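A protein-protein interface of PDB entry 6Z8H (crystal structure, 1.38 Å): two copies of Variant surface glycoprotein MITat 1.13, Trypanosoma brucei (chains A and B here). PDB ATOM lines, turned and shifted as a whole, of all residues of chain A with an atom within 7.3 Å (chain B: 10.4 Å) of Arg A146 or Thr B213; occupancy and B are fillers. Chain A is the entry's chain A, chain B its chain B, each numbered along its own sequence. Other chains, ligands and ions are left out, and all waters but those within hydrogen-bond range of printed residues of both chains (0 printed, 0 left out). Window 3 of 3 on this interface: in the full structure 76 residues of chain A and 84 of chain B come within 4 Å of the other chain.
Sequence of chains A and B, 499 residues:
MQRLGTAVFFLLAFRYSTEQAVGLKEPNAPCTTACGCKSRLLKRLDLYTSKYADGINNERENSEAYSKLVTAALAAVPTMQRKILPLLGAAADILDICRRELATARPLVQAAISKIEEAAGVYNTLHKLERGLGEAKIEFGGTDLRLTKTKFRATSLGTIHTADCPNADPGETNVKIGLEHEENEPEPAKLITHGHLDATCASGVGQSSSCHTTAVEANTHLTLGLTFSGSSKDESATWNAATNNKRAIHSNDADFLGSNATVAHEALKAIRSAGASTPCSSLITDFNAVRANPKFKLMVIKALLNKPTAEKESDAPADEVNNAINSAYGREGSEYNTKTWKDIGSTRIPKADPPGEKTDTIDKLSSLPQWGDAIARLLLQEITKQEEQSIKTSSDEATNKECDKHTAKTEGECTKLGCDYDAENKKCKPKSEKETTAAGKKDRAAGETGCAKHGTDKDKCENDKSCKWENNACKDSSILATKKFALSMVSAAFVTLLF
Of the 23 printed residues of chain B, 10 touch a printed residue of chain A.
Among the printed residues, no Asp or Glu carboxylate lies within 4 Å of a Lys or Arg side-chain nitrogen of the other chain.
The guanidinium group (NH2) of Arg A146 sits at hydrogen-bond distance from the backbone carbonyl oxygen (O) of Thr B213, at 3.0 Å.
The backbone carbonyl oxygen (O) of Leu A145 lies within hydrogen-bond range of the backbone NH (N) of Val B216.
N of Leu A147 is in hydrogen-bond range of O of Cys B211, 2.8 Å away.
Ile A138 touches Leu B222 (CD1 to CD2, 3.9 Å).
CE1 of Phe A140 touches CG2 of Val B216, 3.9 Å away.
Arg A146 touches His B212 (CD to O, 3.2 Å).
Arg A146 touches Ala B215 (N to CB, 3.5 Å).
Leu A147 touches Cys B201 (CD2 to SG, 3.9 Å).
His B212 touches Leu A147 (CA to O, 3.5 Å).
Leu A147 touches Leu B222 (CD2 to CD1, 3.8 Å).
Thr B243 touches Leu A147.
His B212 touches Thr A148.
Thr A148 touches Asn B240.
Asp A144 touches none of the printed residues of chain B.
Leu A145 touches just these residues of chain B: Ala B215 (3.4 Å) and Val B216 (2.7 Å).
Of chain B, only Cys B211 (3.2 Å), His B212 (3.2 Å), Thr B213 (3.0 Å) and Ala B215 (3.5 Å) come within 4 Å of Arg A146.
Leu A147 touches five residues of chain B.
Ser B208 touches none of the printed residues of chain A.
Of chain A, only Arg A146 (3.0 Å) comes within 4 Å of Thr B213.
Of the printed residues of chain A, Ala B215 touches Leu A145 (3.4 Å) and Arg A146 (3.5 Å).
Of the printed residues of chain A, Asn B240 touches Thr A148 (3.5 Å).
Printed residues of chain A within 4 Å of Thr B243: Leu A147 (3.7 Å).
The nearest residue of chain A that does not touch Thr B213 is Leu A147 (5.8 Å).
1 position is printed for both chains.
Of the 16 pairs that touch across the chains among the printed residues, none has its exchanged pair printed and touching as well.
O of Phe A140 lies within hydrogen-bond range of NZ of Lys A151 (2.7 Å).
N of Cys B211 sits at hydrogen-bond distance from OG1 of Thr B243, at 2.8 Å.
The indole nitrogen of Trp B239 lies within hydrogen-bond range of the backbone carbonyl oxygen of Thr B243 (3.0 Å).
The backbone NH of Thr B243 lies within hydrogen-bond range of the side-chain hydroxyl of Ser B210, 2.9 Å away.
SG of Cys B211 is disulfide-bonded to SG of Cys B201, 2.0 Å away.
The backbone NH (N) of Asn B244 is in hydrogen-bond range of the backbone carbonyl oxygen (O) of Cys B201 (3.1 Å).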
ATOM      1  N   ILE A 138      25.390  -3.889  -6.460  1.00  0.00           N
ATOM      2  CA  ILE A 138      24.485  -4.927  -6.941  1.00  0.00           C
ATOM      3  C   ILE A 138      23.988  -5.743  -5.760  1.00  0.00           C
ATOM      4  O   ILE A 138      24.786  -6.224  -4.946  1.00  0.00           O
ATOM      5  CB  ILE A 138      25.195  -5.831  -7.960  1.00  0.00           C
ATOM      6  CG1 ILE A 138      25.574  -5.039  -9.204  1.00  0.00           C
ATOM      7  CG2 ILE A 138      24.310  -7.061  -8.277  1.00  0.00           C
ATOM      8  CD1 ILE A 138      26.585  -5.740 -10.081  1.00  0.00           C
ATOM      9  N   GLU A 139      22.669  -5.898  -5.667  1.00  0.00           N
ATOM     10  CA  GLU A 139      22.038  -6.843  -4.752  1.00  0.00           C
ATOM     11  C   GLU A 139      21.280  -7.840  -5.614  1.00  0.00           C
ATOM     12  O   GLU A 139      20.287  -7.488  -6.254  1.00  0.00           O
ATOM     13  CB  GLU A 139      21.092  -6.120  -3.803  1.00  0.00           C
ATOM     14  CG  GLU A 139      21.691  -4.909  -3.113  1.00  0.00           C
ATOM     15  CD  GLU A 139      20.645  -4.158  -2.320  1.00  0.00           C
ATOM     16  OE1 GLU A 139      19.462  -4.557  -2.394  1.00  0.00           O
ATOM     17  OE2 GLU A 139      21.006  -3.185  -1.625  1.00  0.00           O
ATOM     18  N   PHE A 140      21.761  -9.073  -5.651  1.00  0.00           N
ATOM     19  CA  PHE A 140      21.196 -10.046  -6.583  1.00  0.00           C
ATOM     20  C   PHE A 140      19.748 -10.438  -6.296  1.00  0.00           C
ATOM     21  O   PHE A 140      19.101 -10.991  -7.194  1.00  0.00           O
ATOM     22  CB  PHE A 140      22.119 -11.246  -6.664  1.00  0.00           C
ATOM     23  CG  PHE A 140      23.288 -11.043  -7.586  1.00  0.00           C
ATOM     24  CD1 PHE A 140      23.113 -11.060  -8.965  1.00  0.00           C
ATOM     25  CD2 PHE A 140      24.554 -10.814  -7.080  1.00  0.00           C
ATOM     26  CE1 PHE A 140      24.177 -10.891  -9.816  1.00  0.00           C
ATOM     27  CE2 PHE A 140      25.623 -10.636  -7.923  1.00  0.00           C
ATOM     28  CZ  PHE A 140      25.438 -10.670  -9.297  1.00  0.00           C
ATOM     29  N   GLY A 141      19.200 -10.093  -5.131  1.00  0.00           N
ATOM     30  CA  GLY A 141      17.772 -10.153  -4.902  1.00  0.00           C
ATOM     31  C   GLY A 141      17.271 -11.353  -4.109  1.00  0.00           C
ATOM     32  O   GLY A 141      16.202 -11.259  -3.499  1.00  0.00           O
ATOM     33  N   THR A 143      16.598 -14.515  -5.428  1.00  0.00           N
ATOM     34  CA  THR A 143      15.921 -15.498  -6.259  1.00  0.00           C
ATOM     35  C   THR A 143      16.827 -16.128  -7.300  1.00  0.00           C
ATOM     36  O   THR A 143      16.780 -17.352  -7.488  1.00  0.00           O
ATOM     37  CB  THR A 143      14.720 -14.847  -6.954  1.00  0.00           C
ATOM     38  OG1 THR A 143      13.795 -14.375  -5.965  1.00  0.00           O
ATOM     39  CG2 THR A 143      14.019 -15.847  -7.864  1.00  0.00           C
ATOM     40  N   ASP A 144      17.653 -15.327  -7.977  1.00  0.00           N
ATOM     41  CA  ASP A 144      18.545 -15.857  -8.999  1.00  0.00           C
ATOM     42  C   ASP A 144      19.718 -14.898  -9.178  1.00  0.00           C
ATOM     43  O   ASP A 144      19.790 -13.835  -8.550  1.00  0.00           O
ATOM     44  CB  ASP A 144      17.810 -16.086 -10.325  1.00  0.00           C
ATOM     45  CG  ASP A 144      17.085 -14.838 -10.828  1.00  0.00           C
ATOM     46  OD1 ASP A 144      17.547 -13.704 -10.571  1.00  0.00           O
ATOM     47  OD2 ASP A 144      16.028 -14.989 -11.479  1.00  0.00           O
ATOM     48  N   LEU A 145      20.649 -15.299 -10.046  1.00  0.00           N
ATOM     49  CA  LEU A 145      21.815 -14.486 -10.388  1.00  0.00           C
ATOM     50  C   LEU A 145      21.666 -13.810 -11.750  1.00  0.00           C
ATOM     51  O   LEU A 145      22.664 -13.334 -12.316  1.00  0.00           O
ATOM     52  CB  LEU A 145      23.094 -15.329 -10.369  1.00  0.00           C
ATOM     53  CG  LEU A 145      23.750 -15.771  -9.054  1.00  0.00           C
ATOM     54  CD1 LEU A 145      24.400 -14.584  -8.365  1.00  0.00           C
ATOM     55  CD2 LEU A 145      22.792 -16.498  -8.112  1.00  0.00           C
ATOM     56  N   ARG A 146      20.444 -13.736 -12.283  1.00  0.00           N
ATOM     57  CA  ARG A 146      20.205 -12.879 -13.435  1.00  0.00           C
ATOM     58  C   ARG A 146      20.401 -11.400 -13.046  1.00  0.00           C
ATOM     59  O   ARG A 146      20.376 -11.023 -11.867  1.00  0.00           O
ATOM     60  CB  ARG A 146      18.824 -13.132 -14.030  1.00  0.00           C
ATOM     61  CG  ARG A 146      18.668 -14.565 -14.552  1.00  0.00           C
ATOM     62  CD  ARG A 146      17.386 -14.745 -15.367  1.00  0.00           C
ATOM     63  NE  ARG A 146      17.328 -16.019 -16.085  1.00  0.00           N
ATOM     64  CZ  ARG A 146      16.260 -16.438 -16.747  1.00  0.00           C
ATOM     65  NH1 ARG A 146      15.176 -15.672 -16.798  1.00  0.00           N
ATOM     66  NH2 ARG A 146      16.271 -17.623 -17.356  1.00  0.00           N
ATOM     67  N   LEU A 147      20.608 -10.553 -14.049  1.00  0.00           N
ATOM     68  CA  LEU A 147      20.959  -9.163 -13.783  1.00  0.00           C
ATOM     69  C   LEU A 147      20.217  -8.253 -14.745  1.00  0.00           C
ATOM     70  O   LEU A 147      20.259  -8.461 -15.963  1.00  0.00           O
ATOM     71  CB  LEU A 147      22.478  -8.961 -13.907  1.00  0.00           C
ATOM     72  CG  LEU A 147      23.081  -7.644 -13.403  1.00  0.00           C
ATOM     73  CD1 LEU A 147      22.635  -7.389 -11.993  1.00  0.00           C
ATOM     74  CD2 LEU A 147      24.580  -7.739 -13.496  1.00  0.00           C
ATOM     75  N   THR A 148      19.550  -7.246 -14.181  1.00  0.00           N
ATOM     76  CA  THR A 148      19.100  -6.082 -14.927  1.00  0.00           C
ATOM     77  C   THR A 148      19.410  -4.867 -14.076  1.00  0.00           C
ATOM     78  O   THR A 148      19.878  -4.980 -12.940  1.00  0.00           O
ATOM     79  CB  THR A 148      17.593  -6.084 -15.244  1.00  0.00           C
ATOM     80  OG1 THR A 148      16.846  -5.768 -14.060  1.00  0.00           O
ATOM     81  CG2 THR A 148      17.149  -7.407 -15.865  1.00  0.00           C
ATOM     82  N   LYS A 151      18.622  -4.469 -10.172  1.00  0.00           N
ATOM     83  CA  LYS A 151      19.424  -5.020  -9.088  1.00  0.00           C
ATOM     84  C   LYS A 151      20.585  -4.119  -8.694  1.00  0.00           C
ATOM     85  O   LYS A 151      21.290  -4.417  -7.720  1.00  0.00           O
ATOM     86  CB  LYS A 151      19.920  -6.421  -9.444  1.00  0.00           C
ATOM     87  CG  LYS A 151      18.772  -7.436  -9.621  1.00  0.00           C
ATOM     88  CD  LYS A 151      19.257  -8.859  -9.753  1.00  0.00           C
ATOM     89  CE  LYS A 151      18.112  -9.871  -9.893  1.00  0.00           C
ATOM     90  NZ  LYS A 151      18.626 -11.253  -9.868  1.00  0.00           N
ATOM     91  N   LEU B 145      31.893 -19.376  -9.053  1.00  0.00           N
ATOM     92  CA  LEU B 145      31.544 -17.977  -8.761  1.00  0.00           C
ATOM     93  C   LEU B 145      32.272 -17.445  -7.539  1.00  0.00           C
ATOM     94  O   LEU B 145      31.834 -16.474  -7.043  1.00  0.00           O
ATOM     95  CB  LEU B 145      30.068 -17.965  -8.408  1.00  0.00           C
ATOM     96  CG  LEU B 145      29.117 -17.841  -9.564  1.00  0.00           C
ATOM     97  CD1 LEU B 145      29.092 -16.415 -10.003  1.00  0.00           C
ATOM     98  CD2 LEU B 145      29.520 -18.767 -10.678  1.00  0.00           C
ATOM     99  N   CYS B 201      27.708  -7.189 -18.737  1.00  0.00           N
ATOM    100  CA  CYS B 201      27.569  -8.500 -18.107  1.00  0.00           C
ATOM    101  C   CYS B 201      27.402  -9.493 -19.242  1.00  0.00           C
ATOM    102  O   CYS B 201      26.467  -9.382 -20.040  1.00  0.00           O
ATOM    103  CB  CYS B 201      26.393  -8.513 -17.127  1.00  0.00           C
ATOM    104  SG  CYS B 201      26.286 -10.039 -16.111  1.00  0.00           S
ATOM    105  N   ALA B 202      28.377 -10.377 -19.385  1.00  0.00           N
ATOM    106  CA  ALA B 202      28.369 -11.378 -20.442  1.00  0.00           C
ATOM    107  C   ALA B 202      28.549 -12.753 -19.814  1.00  0.00           C
ATOM    108  O   ALA B 202      29.598 -13.036 -19.223  1.00  0.00           O
ATOM    109  CB  ALA B 202      29.478 -11.090 -21.453  1.00  0.00           C
ATOM    110  N   SER B 203      27.530 -13.608 -19.944  1.00  0.00           N
ATOM    111  CA  SER B 203      27.497 -14.904 -19.287  1.00  0.00           C
ATOM    112  C   SER B 203      27.544 -16.029 -20.316  1.00  0.00           C
ATOM    113  O   SER B 203      27.288 -15.844 -21.512  1.00  0.00           O
ATOM    114  CB  SER B 203      26.252 -15.045 -18.400  1.00  0.00           C
ATOM    115  OG  SER B 203      25.067 -14.764 -19.131  1.00  0.00           O
ATOM    116  N   GLY B 204      27.884 -17.210 -19.831  1.00  0.00           N
ATOM    117  CA  GLY B 204      27.994 -18.370 -20.684  1.00  0.00           C
ATOM    118  C   GLY B 204      29.385 -18.530 -21.270  1.00  0.00           C
ATOM    119  O   GLY B 204      30.196 -17.608 -21.299  1.00  0.00           O
ATOM    120  N   SER B 208      28.876 -15.122 -24.420  1.00  0.00           N
ATOM    121  CA  SER B 208      28.088 -14.868 -25.615  1.00  0.00           C
ATOM    122  C   SER B 208      26.690 -14.345 -25.336  1.00  0.00           C
ATOM    123  O   SER B 208      26.044 -13.840 -26.263  1.00  0.00           O
ATOM    124  CB  SER B 208      27.938 -16.162 -26.421  1.00  0.00           C
ATOM    125  OG  SER B 208      27.170 -17.125 -25.698  1.00  0.00           O
ATOM    126  N   SER B 209      26.204 -14.459 -24.109  1.00  0.00           N
ATOM    127  CA  SER B 209      24.804 -14.201 -23.837  1.00  0.00           C
ATOM    128  C   SER B 209      24.627 -13.096 -22.801  1.00  0.00           C
ATOM    129  O   SER B 209      25.573 -12.653 -22.142  1.00  0.00           O
ATOM    130  CB  SER B 209      24.105 -15.479 -23.363  1.00  0.00           C
ATOM    131  OG  SER B 209      24.240 -16.526 -24.317  1.00  0.00           O
ATOM    132  N   SER B 210      23.381 -12.660 -22.673  1.00  0.00           N
ATOM    133  CA  SER B 210      23.014 -11.605 -21.748  1.00  0.00           C
ATOM    134  C   SER B 210      22.640 -12.185 -20.388  1.00  0.00           C
ATOM    135  O   SER B 210      22.076 -13.276 -20.288  1.00  0.00           O
ATOM    136  CB  SER B 210      21.827 -10.830 -22.305  1.00  0.00           C
ATOM    137  OG  SER B 210      21.311  -9.969 -21.316  1.00  0.00           O
ATOM    138  N   CYS B 211      22.969 -11.448 -19.339  1.00  0.00           N
ATOM    139  CA  CYS B 211      22.695 -11.813 -17.959  1.00  0.00           C
ATOM    140  C   CYS B 211      21.237 -11.629 -17.562  1.00  0.00           C
ATOM    141  O   CYS B 211      20.867 -12.029 -16.453  1.00  0.00           O
ATOM    142  CB  CYS B 211      23.599 -10.985 -17.025  1.00  0.00           C
ATOM    143  SG  CYS B 211      25.310 -11.415 -17.196  1.00  0.00           S
ATOM    144  N   HIS B 212      20.399 -11.030 -18.411  1.00  0.00           N
ATOM    145  CA  HIS B 212      18.994 -10.937 -18.043  1.00  0.00           C
ATOM    146  C   HIS B 212      18.270 -12.264 -18.256  1.00  0.00           C
ATOM    147  O   HIS B 212      17.242 -12.490 -17.630  1.00  0.00           O
ATOM    148  CB  HIS B 212      18.290  -9.787 -18.783  1.00  0.00           C
ATOM    149  CG  HIS B 212      17.813 -10.135 -20.158  1.00  0.00           C
ATOM    150  ND1 HIS B 212      18.672 -10.453 -21.188  1.00  0.00           N
ATOM    151  CD2 HIS B 212      16.563 -10.182 -20.683  1.00  0.00           C
ATOM    152  CE1 HIS B 212      17.971 -10.719 -22.277  1.00  0.00           C
ATOM    153  NE2 HIS B 212      16.689 -10.562 -21.997  1.00  0.00           N
ATOM    154  N   THR B 213      18.799 -13.138 -19.105  1.00  0.00           N
ATOM    155  CA  THR B 213      18.226 -14.450 -19.339  1.00  0.00           C
ATOM    156  C   THR B 213      19.162 -15.582 -18.976  1.00  0.00           C
ATOM    157  O   THR B 213      18.703 -16.713 -18.884  1.00  0.00           O
ATOM    158  CB  THR B 213      17.818 -14.602 -20.810  1.00  0.00           C
ATOM    159  OG1 THR B 213      18.921 -14.295 -21.668  1.00  0.00           O
ATOM    160  CG2 THR B 213      16.632 -13.706 -21.117  1.00  0.00           C
ATOM    161  N   THR B 214      20.451 -15.331 -18.800  1.00  0.00           N
ATOM    162  CA  THR B 214      21.407 -16.329 -18.330  1.00  0.00           C
ATOM    163  C   THR B 214      22.086 -15.792 -17.074  1.00  0.00           C
ATOM    164  O   THR B 214      22.937 -14.901 -17.160  1.00  0.00           O
ATOM    165  CB  THR B 214      22.438 -16.639 -19.415  1.00  0.00           C
ATOM    166  OG1 THR B 214      21.798 -17.278 -20.532  1.00  0.00           O
ATOM    167  CG2 THR B 214      23.512 -17.591 -18.875  1.00  0.00           C
ATOM    168  N   ALA B 215      21.707 -16.322 -15.916  1.00  0.00           N
ATOM    169  CA  ALA B 215      22.207 -15.831 -14.640  1.00  0.00           C
ATOM    170  C   ALA B 215      23.725 -15.853 -14.614  1.00  0.00           C
ATOM    171  O   ALA B 215      24.367 -16.668 -15.284  1.00  0.00           O
ATOM    172  CB  ALA B 215      21.667 -16.722 -13.519  1.00  0.00           C
ATOM    173  N   VAL B 216      24.299 -14.881 -13.892  1.00  0.00           N
ATOM    174  CA  VAL B 216      25.741 -14.793 -13.685  1.00  0.00           C
ATOM    175  C   VAL B 216      26.281 -16.167 -13.305  1.00  0.00           C
ATOM    176  O   VAL B 216      25.883 -16.731 -12.281  1.00  0.00           O
ATOM    177  CB  VAL B 216      26.067 -13.726 -12.618  1.00  0.00           C
ATOM    178  CG1 VAL B 216      27.515 -13.843 -12.203  1.00  0.00           C
ATOM    179  CG2 VAL B 216      25.734 -12.317 -13.135  1.00  0.00           C
ATOM    180  N   GLU B 217      27.159 -16.714 -14.142  1.00  0.00           N
ATOM    181  CA  GLU B 217      27.719 -18.048 -13.938  1.00  0.00           C
ATOM    182  C   GLU B 217      29.244 -17.985 -14.013  1.00  0.00           C
ATOM    183  O   GLU B 217      29.864 -16.919 -13.927  1.00  0.00           O
ATOM    184  CB  GLU B 217      27.063 -19.035 -14.912  1.00  0.00           C
ATOM    185  CG  GLU B 217      27.012 -18.604 -16.364  1.00  0.00           C
ATOM    186  CD  GLU B 217      28.366 -18.660 -17.041  1.00  0.00           C
ATOM    187  OE1 GLU B 217      29.002 -19.738 -17.009  1.00  0.00           O
ATOM    188  OE2 GLU B 217      28.802 -17.616 -17.585  1.00  0.00           O
ATOM    189  N   THR B 220      31.252 -16.006 -16.627  1.00  0.00           N
ATOM    190  CA  THR B 220      30.706 -14.656 -16.771  1.00  0.00           C
ATOM    191  C   THR B 220      31.756 -13.572 -16.537  1.00  0.00           C
ATOM    192  O   THR B 220      32.533 -13.622 -15.579  1.00  0.00           O
ATOM    193  CB  THR B 220      29.546 -14.427 -15.788  1.00  0.00           C
ATOM    194  OG1 THR B 220      28.441 -15.290 -16.113  1.00  0.00           O
ATOM    195  CG2 THR B 220      29.090 -12.926 -15.803  1.00  0.00           C
ATOM    196  N   LEU B 222      31.857  -9.534 -15.686  1.00  0.00           N
ATOM    197  CA  LEU B 222      31.057  -8.419 -15.178  1.00  0.00           C
ATOM    198  C   LEU B 222      31.965  -7.205 -15.083  1.00  0.00           C
ATOM    199  O   LEU B 222      32.938  -7.218 -14.319  1.00  0.00           O
ATOM    200  CB  LEU B 222      30.501  -8.712 -13.788  1.00  0.00           C
ATOM    201  CG  LEU B 222      29.658  -7.638 -13.104  1.00  0.00           C
ATOM    202  CD1 LEU B 222      28.381  -7.363 -13.883  1.00  0.00           C
ATOM    203  CD2 LEU B 222      29.355  -8.062 -11.671  1.00  0.00           C
ATOM    204  N   TRP B 239      19.879  -2.050 -22.412  1.00  0.00           N
ATOM    205  CA  TRP B 239      20.831  -2.893 -21.705  1.00  0.00           C
ATOM    206  C   TRP B 239      20.120  -4.037 -21.007  1.00  0.00           C
ATOM    207  O   TRP B 239      20.649  -5.151 -20.965  1.00  0.00           O
ATOM    208  CB  TRP B 239      21.626  -2.097 -20.681  1.00  0.00           C
ATOM    209  CG  TRP B 239      22.757  -2.845 -20.094  1.00  0.00           C
ATOM    210  CD1 TRP B 239      23.960  -3.099 -20.682  1.00  0.00           C
ATOM    211  CD2 TRP B 239      22.814  -3.436 -18.793  1.00  0.00           C
ATOM    212  NE1 TRP B 239      24.764  -3.794 -19.820  1.00  0.00           N
ATOM    213  CE2 TRP B 239      24.082  -4.023 -18.657  1.00  0.00           C
ATOM    214  CE3 TRP B 239      21.912  -3.542 -17.738  1.00  0.00           C
ATOM    215  CZ2 TRP B 239      24.476  -4.692 -17.499  1.00  0.00           C
ATOM    216  CZ3 TRP B 239      22.322  -4.163 -16.573  1.00  0.00           C
ATOM    217  CH2 TRP B 239      23.578  -4.753 -16.474  1.00  0.00           C
ATOM    218  N   ASN B 240      18.948  -3.771 -20.411  1.00  0.00           N
ATOM    219  CA  ASN B 240      18.214  -4.796 -19.664  1.00  0.00           C
ATOM    220  C   ASN B 240      17.797  -5.990 -20.535  1.00  0.00           C
ATOM    221  O   ASN B 240      17.439  -7.038 -19.989  1.00  0.00           O
ATOM    222  CB  ASN B 240      16.967  -4.171 -19.013  1.00  0.00           C
ATOM    223  CG  ASN B 240      17.294  -3.307 -17.808  1.00  0.00           C
ATOM    224  OD1 ASN B 240      18.412  -3.338 -17.288  1.00  0.00           O
ATOM    225  ND2 ASN B 240      16.301  -2.544 -17.341  1.00  0.00           N
ATOM    226  N   ALA B 241      17.835  -5.858 -21.859  1.00  0.00           N
ATOM    227  CA  ALA B 241      17.521  -6.950 -22.776  1.00  0.00           C
ATOM    228  C   ALA B 241      18.754  -7.464 -23.509  1.00  0.00           C
ATOM    229  O   ALA B 241      18.625  -8.353 -24.373  1.00  0.00           O
ATOM    230  CB  ALA B 241      16.464  -6.492 -23.791  1.00  0.00           C
ATOM    231  N   ALA B 242      19.938  -6.935 -23.191  1.00  0.00           N
ATOM    232  CA  ALA B 242      21.175  -7.401 -23.804  1.00  0.00           C
ATOM    233  C   ALA B 242      22.360  -6.851 -23.009  1.00  0.00           C
ATOM    234  O   ALA B 242      23.015  -5.873 -23.419  1.00  0.00           O
ATOM    235  CB  ALA B 242      21.257  -6.906 -25.244  1.00  0.00           C
ATOM    236  N   THR B 243      22.603  -7.403 -21.829  1.00  0.00           N
ATOM    237  CA  THR B 243      23.589  -6.823 -20.925  1.00  0.00           C
ATOM    238  C   THR B 243      25.012  -7.006 -21.428  1.00  0.00           C
ATOM    239  O   THR B 243      25.920  -6.374 -20.893  1.00  0.00           O
ATOM    240  CB  THR B 243      23.475  -7.440 -19.525  1.00  0.00           C
ATOM    241  OG1 THR B 243      23.879  -8.813 -19.571  1.00  0.00           O
ATOM    242  CG2 THR B 243      22.058  -7.368 -18.999  1.00  0.00           C
ATOM    243  N   ASN B 244      25.233  -7.859 -22.422  1.00  0.00           N
ATOM    244  CA  ASN B 244      26.569  -8.102 -22.951  1.00  0.00           C
ATOM    245  C   ASN B 244      27.065  -6.990 -23.854  1.00  0.00           C
ATOM    246  O   ASN B 244      28.134  -7.113 -24.465  1.00  0.00           O
ATOM    247  CB  ASN B 244      26.660  -9.487 -23.632  1.00  0.00           C
ATOM    248  CG  ASN B 244      25.560  -9.765 -24.684  1.00  0.00           C
ATOM    249  OD1 ASN B 244      24.429  -9.303 -24.591  1.00  0.00           O
ATOM    250  ND2 ASN B 244      25.905 -10.612 -25.663  1.00  0.00           N
